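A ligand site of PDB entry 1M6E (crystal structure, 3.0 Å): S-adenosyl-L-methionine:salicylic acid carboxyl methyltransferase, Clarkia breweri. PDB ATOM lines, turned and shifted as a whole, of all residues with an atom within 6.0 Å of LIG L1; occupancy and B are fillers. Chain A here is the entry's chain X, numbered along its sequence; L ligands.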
ATOM      1  N   HIS A   8      28.267  23.156 -11.222  1.00  0.00           N
ATOM      2  CA  HIS A   8      27.385  23.209 -10.084  1.00  0.00           C
ATOM      3  C   HIS A   8      27.704  24.065  -8.877  1.00  0.00           C
ATOM      4  O   HIS A   8      28.862  24.288  -8.472  1.00  0.00           O
ATOM      5  CB  HIS A   8      27.030  21.806  -9.591  1.00  0.00           C
ATOM      6  CG  HIS A   8      27.968  21.240  -8.586  1.00  0.00           C
ATOM      7  ND1 HIS A   8      27.624  20.181  -7.773  1.00  0.00           N
ATOM      8  CD2 HIS A   8      29.244  21.570  -8.263  1.00  0.00           C
ATOM      9  CE1 HIS A   8      28.642  19.884  -6.978  1.00  0.00           C
ATOM     10  NE2 HIS A   8      29.638  20.713  -7.256  1.00  0.00           N
ATOM     11  N   MET A   9      26.585  24.526  -8.317  1.00  0.00           N
ATOM     12  CA  MET A   9      26.499  25.364  -7.140  1.00  0.00           C
ATOM     13  C   MET A   9      25.035  25.148  -6.738  1.00  0.00           C
ATOM     14  O   MET A   9      24.329  24.409  -7.400  1.00  0.00           O
ATOM     15  CB  MET A   9      26.743  26.829  -7.494  1.00  0.00           C
ATOM     16  CG  MET A   9      25.575  27.516  -8.237  1.00  0.00           C
ATOM     17  SD  MET A   9      25.677  27.377 -10.017  1.00  0.00           S
ATOM     18  CE  MET A   9      24.350  28.525 -10.523  1.00  0.00           C
ATOM     19  N   LYS A  10      24.596  25.802  -5.670  1.00  0.00           N
ATOM     20  CA  LYS A  10      23.225  25.667  -5.185  1.00  0.00           C
ATOM     21  C   LYS A  10      22.537  26.932  -5.595  1.00  0.00           C
ATOM     22  O   LYS A  10      23.232  27.894  -5.904  1.00  0.00           O
ATOM     23  CB  LYS A  10      23.238  25.570  -3.656  1.00  0.00           C
ATOM     24  CG  LYS A  10      24.187  24.527  -3.106  1.00  0.00           C
ATOM     25  CD  LYS A  10      23.524  23.217  -2.957  1.00  0.00           C
ATOM     26  CE  LYS A  10      24.472  22.136  -3.314  1.00  0.00           C
ATOM     27  NZ  LYS A  10      24.703  22.408  -4.732  1.00  0.00           N
ATOM     28  N   TYR A  18      17.925  27.718  -1.684  1.00  0.00           N
ATOM     29  CA  TYR A  18      19.133  27.525  -0.850  1.00  0.00           C
ATOM     30  C   TYR A  18      19.538  28.678   0.022  1.00  0.00           C
ATOM     31  O   TYR A  18      20.461  29.462  -0.291  1.00  0.00           O
ATOM     32  CB  TYR A  18      20.339  27.094  -1.684  1.00  0.00           C
ATOM     33  CG  TYR A  18      21.251  26.229  -0.838  1.00  0.00           C
ATOM     34  CD1 TYR A  18      21.220  24.847  -0.931  1.00  0.00           C
ATOM     35  CD2 TYR A  18      21.979  26.780   0.205  1.00  0.00           C
ATOM     36  CE1 TYR A  18      21.876  24.036  -0.006  1.00  0.00           C
ATOM     37  CE2 TYR A  18      22.633  25.976   1.124  1.00  0.00           C
ATOM     38  CZ  TYR A  18      22.561  24.614   1.007  1.00  0.00           C
ATOM     39  OH  TYR A  18      23.145  23.828   1.957  1.00  0.00           O
ATOM     40  N   SER A  22      17.423  25.073   3.129  1.00  0.00           N
ATOM     41  CA  SER A  22      18.470  24.197   3.608  1.00  0.00           C
ATOM     42  C   SER A  22      18.415  23.956   5.098  1.00  0.00           C
ATOM     43  O   SER A  22      19.455  23.950   5.758  1.00  0.00           O
ATOM     44  CB  SER A  22      19.834  24.761   3.222  1.00  0.00           C
ATOM     45  OG  SER A  22      19.951  26.077   3.683  1.00  0.00           O
ATOM     46  N   GLN A  25      20.148  20.452   6.208  1.00  0.00           N
ATOM     47  CA  GLN A  25      21.604  20.440   6.351  1.00  0.00           C
ATOM     48  C   GLN A  25      21.945  21.264   7.593  1.00  0.00           C
ATOM     49  O   GLN A  25      23.019  21.120   8.197  1.00  0.00           O
ATOM     50  CB  GLN A  25      22.296  20.997   5.108  1.00  0.00           C
ATOM     51  CG  GLN A  25      21.387  21.787   4.196  1.00  0.00           C
ATOM     52  CD  GLN A  25      20.744  20.914   3.153  1.00  0.00           C
ATOM     53  OE1 GLN A  25      19.535  20.980   2.927  1.00  0.00           O
ATOM     54  NE2 GLN A  25      21.563  20.095   2.492  1.00  0.00           N
ATOM     55  N   ARG A  26      21.003  22.124   7.982  1.00  0.00           N
ATOM     56  CA  ARG A  26      21.203  22.959   9.153  1.00  0.00           C
ATOM     57  C   ARG A  26      21.085  22.195  10.440  1.00  0.00           C
ATOM     58  O   ARG A  26      21.756  22.530  11.394  1.00  0.00           O
ATOM     59  CB  ARG A  26      20.188  24.098   9.187  1.00  0.00           C
ATOM     60  CG  ARG A  26      20.475  25.069  10.305  1.00  0.00           C
ATOM     61  CD  ARG A  26      19.946  26.415   9.920  1.00  0.00           C
ATOM     62  NE  ARG A  26      20.617  27.509  10.598  1.00  0.00           N
ATOM     63  CZ  ARG A  26      20.534  27.743  11.898  1.00  0.00           C
ATOM     64  NH1 ARG A  26      19.788  26.949  12.679  1.00  0.00           N
ATOM     65  NH2 ARG A  26      21.165  28.787  12.416  1.00  0.00           N
ATOM     66  N   ILE A  29      24.124  20.006  11.052  1.00  0.00           N
ATOM     67  CA  ILE A  29      25.245  20.742  11.614  1.00  0.00           C
ATOM     68  C   ILE A  29      25.033  20.945  13.111  1.00  0.00           C
ATOM     69  O   ILE A  29      26.002  21.063  13.885  1.00  0.00           O
ATOM     70  CB  ILE A  29      25.435  22.127  10.937  1.00  0.00           C
ATOM     71  CG1 ILE A  29      25.768  21.931   9.446  1.00  0.00           C
ATOM     72  CG2 ILE A  29      26.513  22.934  11.681  1.00  0.00           C
ATOM     73  CD1 ILE A  29      25.711  23.178   8.562  1.00  0.00           C
ATOM     74  N   ASP A  57      35.669  26.739   6.558  1.00  0.00           N
ATOM     75  CA  ASP A  57      34.556  25.879   6.118  1.00  0.00           C
ATOM     76  C   ASP A  57      34.750  25.482   4.646  1.00  0.00           C
ATOM     77  O   ASP A  57      34.954  26.320   3.785  1.00  0.00           O
ATOM     78  CB  ASP A  57      33.190  26.572   6.293  1.00  0.00           C
ATOM     79  CG  ASP A  57      31.993  25.567   6.336  1.00  0.00           C
ATOM     80  OD1 ASP A  57      31.769  24.778   5.376  1.00  0.00           O
ATOM     81  OD2 ASP A  57      31.260  25.561   7.368  1.00  0.00           O
ATOM     82  N   LEU A  58      34.716  24.190   4.362  1.00  0.00           N
ATOM     83  CA  LEU A  58      34.907  23.713   3.017  1.00  0.00           C
ATOM     84  C   LEU A  58      33.591  23.259   2.425  1.00  0.00           C
ATOM     85  O   LEU A  58      32.933  22.351   2.958  1.00  0.00           O
ATOM     86  CB  LEU A  58      35.938  22.570   3.034  1.00  0.00           C
ATOM     87  CG  LEU A  58      37.378  22.928   2.611  1.00  0.00           C
ATOM     88  CD1 LEU A  58      37.721  24.382   2.860  1.00  0.00           C
ATOM     89  CD2 LEU A  58      38.329  22.042   3.358  1.00  0.00           C
ATOM     90  N   GLY A  59      33.194  23.905   1.328  1.00  0.00           N
ATOM     91  CA  GLY A  59      31.941  23.591   0.681  1.00  0.00           C
ATOM     92  C   GLY A  59      30.810  24.258   1.435  1.00  0.00           C
ATOM     93  O   GLY A  59      29.754  23.673   1.664  1.00  0.00           O
ATOM     94  N   CYS A  60      31.061  25.502   1.858  1.00  0.00           N
ATOM     95  CA  CYS A  60      30.061  26.303   2.570  1.00  0.00           C
ATOM     96  C   CYS A  60      29.113  26.655   1.460  1.00  0.00           C
ATOM     97  O   CYS A  60      29.213  26.089   0.387  1.00  0.00           O
ATOM     98  CB  CYS A  60      30.699  27.596   3.110  1.00  0.00           C
ATOM     99  SG  CYS A  60      31.348  28.748   1.810  1.00  0.00           S
ATOM    100  N   SER A  61      28.201  27.582   1.666  1.00  0.00           N
ATOM    101  CA  SER A  61      27.375  27.880   0.526  1.00  0.00           C
ATOM    102  C   SER A  61      26.948  29.321   0.465  1.00  0.00           C
ATOM    103  O   SER A  61      27.771  30.199   0.260  1.00  0.00           O
ATOM    104  CB  SER A  61      26.174  26.973   0.495  1.00  0.00           C
ATOM    105  OG  SER A  61      25.894  26.689  -0.856  1.00  0.00           O
ATOM    106  N   PRO A  64      22.578  31.260   5.553  1.00  0.00           N
ATOM    107  CA  PRO A  64      23.076  30.696   6.820  1.00  0.00           C
ATOM    108  C   PRO A  64      23.847  29.432   6.516  1.00  0.00           C
ATOM    109  O   PRO A  64      23.941  29.043   5.350  1.00  0.00           O
ATOM    110  CB  PRO A  64      21.791  30.437   7.579  1.00  0.00           C
ATOM    111  CG  PRO A  64      20.844  31.467   6.985  1.00  0.00           C
ATOM    112  CD  PRO A  64      21.121  31.343   5.546  1.00  0.00           C
ATOM    113  N   ASN A  65      24.387  28.793   7.550  1.00  0.00           N
ATOM    114  CA  ASN A  65      25.180  27.561   7.424  1.00  0.00           C
ATOM    115  C   ASN A  65      26.603  27.886   7.003  1.00  0.00           C
ATOM    116  O   ASN A  65      27.555  27.331   7.546  1.00  0.00           O
ATOM    117  CB  ASN A  65      24.572  26.559   6.427  1.00  0.00           C
ATOM    118  CG  ASN A  65      23.068  26.392   6.579  1.00  0.00           C
ATOM    119  OD1 ASN A  65      22.304  26.894   5.742  1.00  0.00           O
ATOM    120  ND2 ASN A  65      22.632  25.725   7.637  1.00  0.00           N
ATOM    121  N   ALA A  66      26.753  28.774   6.035  1.00  0.00           N
ATOM    122  CA  ALA A  66      28.082  29.154   5.603  1.00  0.00           C
ATOM    123  C   ALA A  66      28.858  29.517   6.865  1.00  0.00           C
ATOM    124  O   ALA A  66      29.920  28.965   7.140  1.00  0.00           O
ATOM    125  CB  ALA A  66      28.010  30.342   4.647  1.00  0.00           C
ATOM    126  N   ASN A  97      35.062  28.444   1.734  1.00  0.00           N
ATOM    127  CA  ASN A  97      35.392  27.874   0.449  1.00  0.00           C
ATOM    128  C   ASN A  97      34.297  27.205  -0.338  1.00  0.00           C
ATOM    129  O   ASN A  97      33.464  26.446   0.180  1.00  0.00           O
ATOM    130  CB  ASN A  97      36.534  26.854   0.585  1.00  0.00           C
ATOM    131  CG  ASN A  97      36.601  25.904  -0.615  1.00  0.00           C
ATOM    132  OD1 ASN A  97      36.001  24.811  -0.620  1.00  0.00           O
ATOM    133  ND2 ASN A  97      37.316  26.322  -1.636  1.00  0.00           N
ATOM    134  N   ASP A  98      34.310  27.484  -1.622  1.00  0.00           N
ATOM    135  CA  ASP A  98      33.355  26.842  -2.448  1.00  0.00           C
ATOM    136  C   ASP A  98      33.815  26.969  -3.852  1.00  0.00           C
ATOM    137  O   ASP A  98      34.837  27.626  -4.098  1.00  0.00           O
ATOM    138  CB  ASP A  98      31.974  27.422  -2.253  1.00  0.00           C
ATOM    139  CG  ASP A  98      30.914  26.453  -2.677  1.00  0.00           C
ATOM    140  OD1 ASP A  98      30.893  26.127  -3.885  1.00  0.00           O
ATOM    141  OD2 ASP A  98      30.128  25.984  -1.820  1.00  0.00           O
ATOM    142  N   LEU A  99      33.095  26.320  -4.777  1.00  0.00           N
ATOM    143  CA  LEU A  99      33.493  26.366  -6.169  1.00  0.00           C
ATOM    144  C   LEU A  99      33.259  27.768  -6.666  1.00  0.00           C
ATOM    145  O   LEU A  99      32.458  28.513  -6.090  1.00  0.00           O
ATOM    146  CB  LEU A  99      32.681  25.376  -6.999  1.00  0.00           C
ATOM    147  CG  LEU A  99      33.069  23.940  -6.719  1.00  0.00           C
ATOM    148  CD1 LEU A  99      32.236  23.034  -7.542  1.00  0.00           C
ATOM    149  CD2 LEU A  99      34.535  23.737  -7.012  1.00  0.00           C
ATOM    150  N   ASN A 102      29.669  30.254  -6.779  1.00  0.00           N
ATOM    151  CA  ASN A 102      28.786  29.919  -5.679  1.00  0.00           C
ATOM    152  C   ASN A 102      28.322  31.368  -5.400  1.00  0.00           C
ATOM    153  O   ASN A 102      28.735  32.280  -6.109  1.00  0.00           O
ATOM    154  CB  ASN A 102      29.585  29.374  -4.507  1.00  0.00           C
ATOM    155  CG  ASN A 102      28.843  29.512  -3.180  1.00  0.00           C
ATOM    156  OD1 ASN A 102      27.660  29.107  -3.072  1.00  0.00           O
ATOM    157  ND2 ASN A 102      29.526  30.097  -2.174  1.00  0.00           N
ATOM    158  N   GLY A 128      37.354  27.768  -5.163  1.00  0.00           N
ATOM    159  CA  GLY A 128      38.124  26.680  -5.733  1.00  0.00           C
ATOM    160  C   GLY A 128      37.674  25.317  -5.267  1.00  0.00           C
ATOM    161  O   GLY A 128      36.851  25.201  -4.379  1.00  0.00           O
ATOM    162  N   SER A 129      38.235  24.274  -5.874  1.00  0.00           N
ATOM    163  CA  SER A 129      37.859  22.931  -5.506  1.00  0.00           C
ATOM    164  C   SER A 129      38.730  22.433  -4.371  1.00  0.00           C
ATOM    165  O   SER A 129      39.917  22.695  -4.330  1.00  0.00           O
ATOM    166  CB  SER A 129      37.983  22.026  -6.708  1.00  0.00           C
ATOM    167  OG  SER A 129      37.565  20.713  -6.383  1.00  0.00           O
ATOM    168  N   PHE A 130      38.109  21.726  -3.438  1.00  0.00           N
ATOM    169  CA  PHE A 130      38.862  21.215  -2.302  1.00  0.00           C
ATOM    170  C   PHE A 130      39.475  19.891  -2.701  1.00  0.00           C
ATOM    171  O   PHE A 130      39.922  19.096  -1.860  1.00  0.00           O
ATOM    172  CB  PHE A 130      37.975  21.098  -1.027  1.00  0.00           C
ATOM    173  CG  PHE A 130      36.662  20.374  -1.214  1.00  0.00           C
ATOM    174  CD1 PHE A 130      36.559  19.220  -1.990  1.00  0.00           C
ATOM    175  CD2 PHE A 130      35.506  20.869  -0.604  1.00  0.00           C
ATOM    176  CE1 PHE A 130      35.316  18.580  -2.173  1.00  0.00           C
ATOM    177  CE2 PHE A 130      34.252  20.247  -0.779  1.00  0.00           C
ATOM    178  CZ  PHE A 130      34.163  19.094  -1.575  1.00  0.00           C
ATOM    179  N   TYR A 131      39.477  19.639  -4.004  1.00  0.00           N
ATOM    180  CA  TYR A 131      40.096  18.419  -4.491  1.00  0.00           C
ATOM    181  C   TYR A 131      41.328  19.019  -5.150  1.00  0.00           C
ATOM    182  O   TYR A 131      41.548  18.905  -6.343  1.00  0.00           O
ATOM    183  CB  TYR A 131      39.203  17.654  -5.518  1.00  0.00           C
ATOM    184  CG  TYR A 131      38.054  16.860  -4.901  1.00  0.00           C
ATOM    185  CD1 TYR A 131      36.751  16.989  -5.373  1.00  0.00           C
ATOM    186  CD2 TYR A 131      38.251  16.009  -3.814  1.00  0.00           C
ATOM    187  CE1 TYR A 131      35.664  16.301  -4.773  1.00  0.00           C
ATOM    188  CE2 TYR A 131      37.179  15.312  -3.213  1.00  0.00           C
ATOM    189  CZ  TYR A 131      35.880  15.484  -3.701  1.00  0.00           C
ATOM    190  OH  TYR A 131      34.832  14.870  -3.081  1.00  0.00           O
ATOM    191  N   HIS A 144      36.149  22.693   9.032  1.00  0.00           N
ATOM    192  CA  HIS A 144      34.810  22.143   9.150  1.00  0.00           C
ATOM    193  C   HIS A 144      34.249  21.732   7.769  1.00  0.00           C
ATOM    194  O   HIS A 144      34.724  22.232   6.775  1.00  0.00           O
ATOM    195  CB  HIS A 144      33.861  23.149   9.820  1.00  0.00           C
ATOM    196  CG  HIS A 144      32.472  22.614   9.927  1.00  0.00           C
ATOM    197  ND1 HIS A 144      31.484  22.933   9.023  1.00  0.00           N
ATOM    198  CD2 HIS A 144      31.982  21.595  10.672  1.00  0.00           C
ATOM    199  CE1 HIS A 144      30.452  22.139   9.202  1.00  0.00           C
ATOM    200  NE2 HIS A 144      30.731  21.313  10.193  1.00  0.00           N
ATOM    201  N   SER A 145      33.267  20.829   7.704  1.00  0.00           N
ATOM    202  CA  SER A 145      32.679  20.486   6.407  1.00  0.00           C
ATOM    203  C   SER A 145      31.479  19.590   6.340  1.00  0.00           C
ATOM    204  O   SER A 145      31.630  18.381   6.258  1.00  0.00           O
ATOM    205  CB  SER A 145      33.721  19.882   5.450  1.00  0.00           C
ATOM    206  OG  SER A 145      33.046  19.350   4.300  1.00  0.00           O
ATOM    207  N   SER A 146      30.282  20.153   6.296  1.00  0.00           N
ATOM    208  CA  SER A 146      29.082  19.325   6.152  1.00  0.00           C
ATOM    209  C   SER A 146      28.626  19.181   4.684  1.00  0.00           C
ATOM    210  O   SER A 146      29.034  19.934   3.806  1.00  0.00           O
ATOM    211  CB  SER A 146      27.927  19.879   6.990  1.00  0.00           C
ATOM    212  OG  SER A 146      27.944  19.334   8.295  1.00  0.00           O
ATOM    213  N   TYR A 147      27.776  18.181   4.464  1.00  0.00           N
ATOM    214  CA  TYR A 147      27.184  17.844   3.174  1.00  0.00           C
ATOM    215  C   TYR A 147      27.795  18.353   1.880  1.00  0.00           C
ATOM    216  O   TYR A 147      27.083  18.785   0.947  1.00  0.00           O
ATOM    217  CB  TYR A 147      25.710  18.234   3.216  1.00  0.00           C
ATOM    218  CG  TYR A 147      24.827  17.246   3.916  1.00  0.00           C
ATOM    219  CD1 TYR A 147      23.570  16.962   3.408  1.00  0.00           C
ATOM    220  CD2 TYR A 147      25.239  16.573   5.069  1.00  0.00           C
ATOM    221  CE1 TYR A 147      22.739  16.015   4.012  1.00  0.00           C
ATOM    222  CE2 TYR A 147      24.416  15.629   5.688  1.00  0.00           C
ATOM    223  CZ  TYR A 147      23.159  15.355   5.145  1.00  0.00           C
ATOM    224  OH  TYR A 147      22.295  14.442   5.706  1.00  0.00           O
ATOM    225  N   SER A 148      29.125  18.306   1.792  1.00  0.00           N
ATOM    226  CA  SER A 148      29.754  18.756   0.579  1.00  0.00           C
ATOM    227  C   SER A 148      30.737  17.718   0.074  1.00  0.00           C
ATOM    228  O   SER A 148      30.959  17.582  -1.129  1.00  0.00           O
ATOM    229  CB  SER A 148      30.477  20.050   0.800  1.00  0.00           C
ATOM    230  OG  SER A 148      31.738  19.799   1.353  1.00  0.00           O
ATOM    231  N   TRP A 151      30.154  15.158  -2.957  1.00  0.00           N
ATOM    232  CA  TRP A 151      30.189  15.621  -4.324  1.00  0.00           C
ATOM    233  C   TRP A 151      31.497  15.204  -4.923  1.00  0.00           C
ATOM    234  O   TRP A 151      32.570  15.297  -4.291  1.00  0.00           O
ATOM    235  CB  TRP A 151      30.039  17.119  -4.386  1.00  0.00           C
ATOM    236  CG  TRP A 151      28.650  17.511  -4.177  1.00  0.00           C
ATOM    237  CD1 TRP A 151      28.165  18.224  -3.150  1.00  0.00           C
ATOM    238  CD2 TRP A 151      27.559  17.273  -5.078  1.00  0.00           C
ATOM    239  NE1 TRP A 151      26.829  18.461  -3.340  1.00  0.00           N
ATOM    240  CE2 TRP A 151      26.428  17.889  -4.516  1.00  0.00           C
ATOM    241  CE3 TRP A 151      27.433  16.599  -6.301  1.00  0.00           C
ATOM    242  CZ2 TRP A 151      25.170  17.867  -5.137  1.00  0.00           C
ATOM    243  CZ3 TRP A 151      26.177  16.570  -6.916  1.00  0.00           C
ATOM    244  CH2 TRP A 151      25.053  17.211  -6.328  1.00  0.00           C
ATOM    245  N   LEU A 152      31.421  14.748  -6.158  1.00  0.00           N
ATOM    246  CA  LEU A 152      32.614  14.283  -6.811  1.00  0.00           C
ATOM    247  C   LEU A 152      33.387  15.310  -7.654  1.00  0.00           C
ATOM    248  O   LEU A 152      32.911  16.400  -7.984  1.00  0.00           O
ATOM    249  CB  LEU A 152      32.260  13.068  -7.663  1.00  0.00           C
ATOM    250  CG  LEU A 152      32.017  11.762  -6.911  1.00  0.00           C
ATOM    251  CD1 LEU A 152      31.491  10.745  -7.880  1.00  0.00           C
ATOM    252  CD2 LEU A 152      33.325  11.308  -6.290  1.00  0.00           C
ATOM    253  N   SER A 153      34.616  14.953  -7.961  1.00  0.00           N
ATOM    254  CA  SER A 153      35.475  15.761  -8.786  1.00  0.00           C
ATOM    255  C   SER A 153      34.814  15.856 -10.161  1.00  0.00           C
ATOM    256  O   SER A 153      34.756  16.925 -10.765  1.00  0.00           O
ATOM    257  CB  SER A 153      36.868  15.101  -8.875  1.00  0.00           C
ATOM    258  OG  SER A 153      37.503  15.175 -10.146  1.00  0.00           O
HETATM  259  N1  LIG L   1      27.900  23.248   4.054  1.00  0.00           N
HETATM  260  C1  LIG L   1      26.432  23.684   3.916  1.00  0.00           C
HETATM  261  C2  LIG L   1      25.816  23.380   2.534  1.00  0.00           C
HETATM  262  C3  LIG L   1      26.705  22.779   1.533  1.00  0.00           C
HETATM  263  S1  LIG L   1      26.025  22.371  -0.103  1.00  0.00           S
HETATM  264  C4  LIG L   1      25.485  22.981   4.887  1.00  0.00           C
HETATM  265  O1  LIG L   1      25.937  22.119   5.699  1.00  0.00           O
HETATM  266  O2  LIG L   1      24.245  23.359   4.780  1.00  0.00           O
HETATM  267  C5  LIG L   1      27.552  21.818  -0.795  1.00  0.00           C
HETATM  268  C6  LIG L   1      28.502  22.911  -1.470  1.00  0.00           C
HETATM  269  O3  LIG L   1      29.635  22.078  -1.857  1.00  0.00           O
HETATM  270  C7  LIG L   1      27.968  23.431  -2.861  1.00  0.00           C
HETATM  271  O4  LIG L   1      27.687  24.949  -2.805  1.00  0.00           O
HETATM  272  C8  LIG L   1      29.050  23.190  -3.806  1.00  0.00           C
HETATM  273  O5  LIG L   1      29.376  24.115  -4.787  1.00  0.00           O
HETATM  274  C9  LIG L   1      30.221  22.690  -2.833  1.00  0.00           C
HETATM  275  N2  LIG L   1      31.175  21.865  -3.539  1.00  0.00           N
HETATM  276  C10 LIG L   1      30.991  20.768  -4.345  1.00  0.00           C
HETATM  277  N3  LIG L   1      32.087  20.291  -4.852  1.00  0.00           N
HETATM  278  C11 LIG L   1      33.050  21.133  -4.344  1.00  0.00           C
HETATM  279  C12 LIG L   1      34.452  21.190  -4.499  1.00  0.00           C
HETATM  280  N4  LIG L   1      35.084  20.306  -5.266  1.00  0.00           N
HETATM  281  N5  LIG L   1      35.186  22.168  -3.849  1.00  0.00           N
HETATM  282  C13 LIG L   1      34.519  23.073  -3.062  1.00  0.00           C
HETATM  283  N6  LIG L   1      33.175  23.105  -2.848  1.00  0.00           N
HETATM  284  C14 LIG L   1      32.493  22.101  -3.531  1.00  0.00           C
HETATM  285  C1  LG2 L   2      23.324  18.246  -1.141  1.00  0.00           C
HETATM  286  O1  LG2 L   2      23.153  19.107  -0.271  1.00  0.00           O
HETATM  287  O2  LG2 L   2      24.369  18.425  -1.984  1.00  0.00           O
HETATM  288  C2  LG2 L   2      22.373  17.064  -1.215  1.00  0.00           C
HETATM  289  C3  LG2 L   2      22.470  15.988  -2.211  1.00  0.00           C
HETATM  290  C4  LG2 L   2      21.511  14.939  -2.170  1.00  0.00           C
HETATM  291  C5  LG2 L   2      20.457  14.875  -1.214  1.00  0.00           C
HETATM  292  C6  LG2 L   2      20.319  15.883  -0.244  1.00  0.00           C
HETATM  293  C7  LG2 L   2      21.326  17.027  -0.248  1.00  0.00           C
HETATM  294  O3  LG2 L   2      23.415  15.894  -3.190  1.00  0.00           O
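The side-chain carboxylate (OD1) of Asp 98 sits at hydrogen-bond distance from an oxygen (O5) of LIG L1, at 2.7 Å.
A nitrogen (N4) of LIG L1 is in hydrogen-bond range of the side-chain hydroxyl of Ser 129 (2.8 Å).
The side-chain hydroxyl of Tyr 18 lies close to an oxygen (O2) of LIG L1.
N5 of LIG L1 sits at hydrogen-bond distance from N of Phe 130, 3.0 Å away.
N1 of LIG L1 is in hydrogen-bond range of O of Gly 59.
OG of Ser 61 sits at hydrogen-bond distance from O4 of LIG L1.
NE2 of His 8 lies close to N3 of LIG L1 (3.5 Å).
O1 of LG2 L2 is in hydrogen-bond range of NE2 of Gln 25, 3.3 Å away.
An oxygen (O2) of LG2 L2 is in hydrogen-bond range of the indole nitrogen (NE1) of Trp 151, 2.8 Å away.
OG of Ser 129 lies close to N of Tyr 131.
The backbone carbonyl oxygen of Asn 97 lies within hydrogen-bond range of the backbone NH of Gly 59.
The backbone carbonyl oxygen of Ser 61 is in hydrogen-bond range of the side-chain amide nitrogen of Asn 102, 3.0 Å away.
The backbone carbonyl oxygen of Gly 128 is in hydrogen-bond range of the side-chain amide nitrogen of Asn 97, at 3.0 Å.
The backbone NH (N) of Cys 60 is in hydrogen-bond range of the backbone carbonyl oxygen (O) of Asn 97, at 3.1 Å.
O of Asp 57 sits at hydrogen-bond distance from N of Asn 97 (3.0 Å).
The side-chain amide oxygen of Asn 65 sits at hydrogen-bond distance from the side-chain hydroxyl of Ser 22 (3.2 Å).
The side-chain hydroxyl (OH) of Tyr 131 sits at hydrogen-bond distance from the backbone carbonyl oxygen (O) of Trp 151, at 2.6 Å.
Met 9 touches LIG L1.
Lys 10 touches LIG L1 (CG to O4, 3.5 Å).
CB of Gln 25 touches O2 of LIG L1 (3.1 Å).
CD1 of Ile 29 touches O1 of LIG L1 (3.1 Å).
O of Cys 60 touches O4 of LIG L1, 3.7 Å away.
Asn 65 touches LIG L1.
OD1 of Asn 97 touches C13 of LIG L1 (3.3 Å).
Leu 99 touches LIG L1.
Gly 128 touches LIG L1.
Tyr 131 touches LIG L1.
Ser 146 touches LIG L1.
Tyr 147 touches LIG L1.
Ser 148 touches LIG L1.
Trp 151 touches LIG L1.
Hydrophobic or aromatic side chains that line LIG L1: His 8, Tyr 18, Ile 29, Leu 99, Phe 130, Tyr 131 and Trp 151.
Within 4 Å of LIG L1: His 8, Met 9, Lys 10, Tyr 18, Gln 25, Ile 29, Gly 59, Cys 60, Ser 61, Asn 65, Asn 97, Asp 98, Leu 99, Gly 128, Ser 129, Phe 130, Tyr 131, Ser 146, Tyr 147, Ser 148 and Trp 151.
Along chain A the residues within 4 Å of LIG L1 span positions 8 to 151.
The nearest printed residue that does not touch LIG L1 is Asn 102 (4.2 Å).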
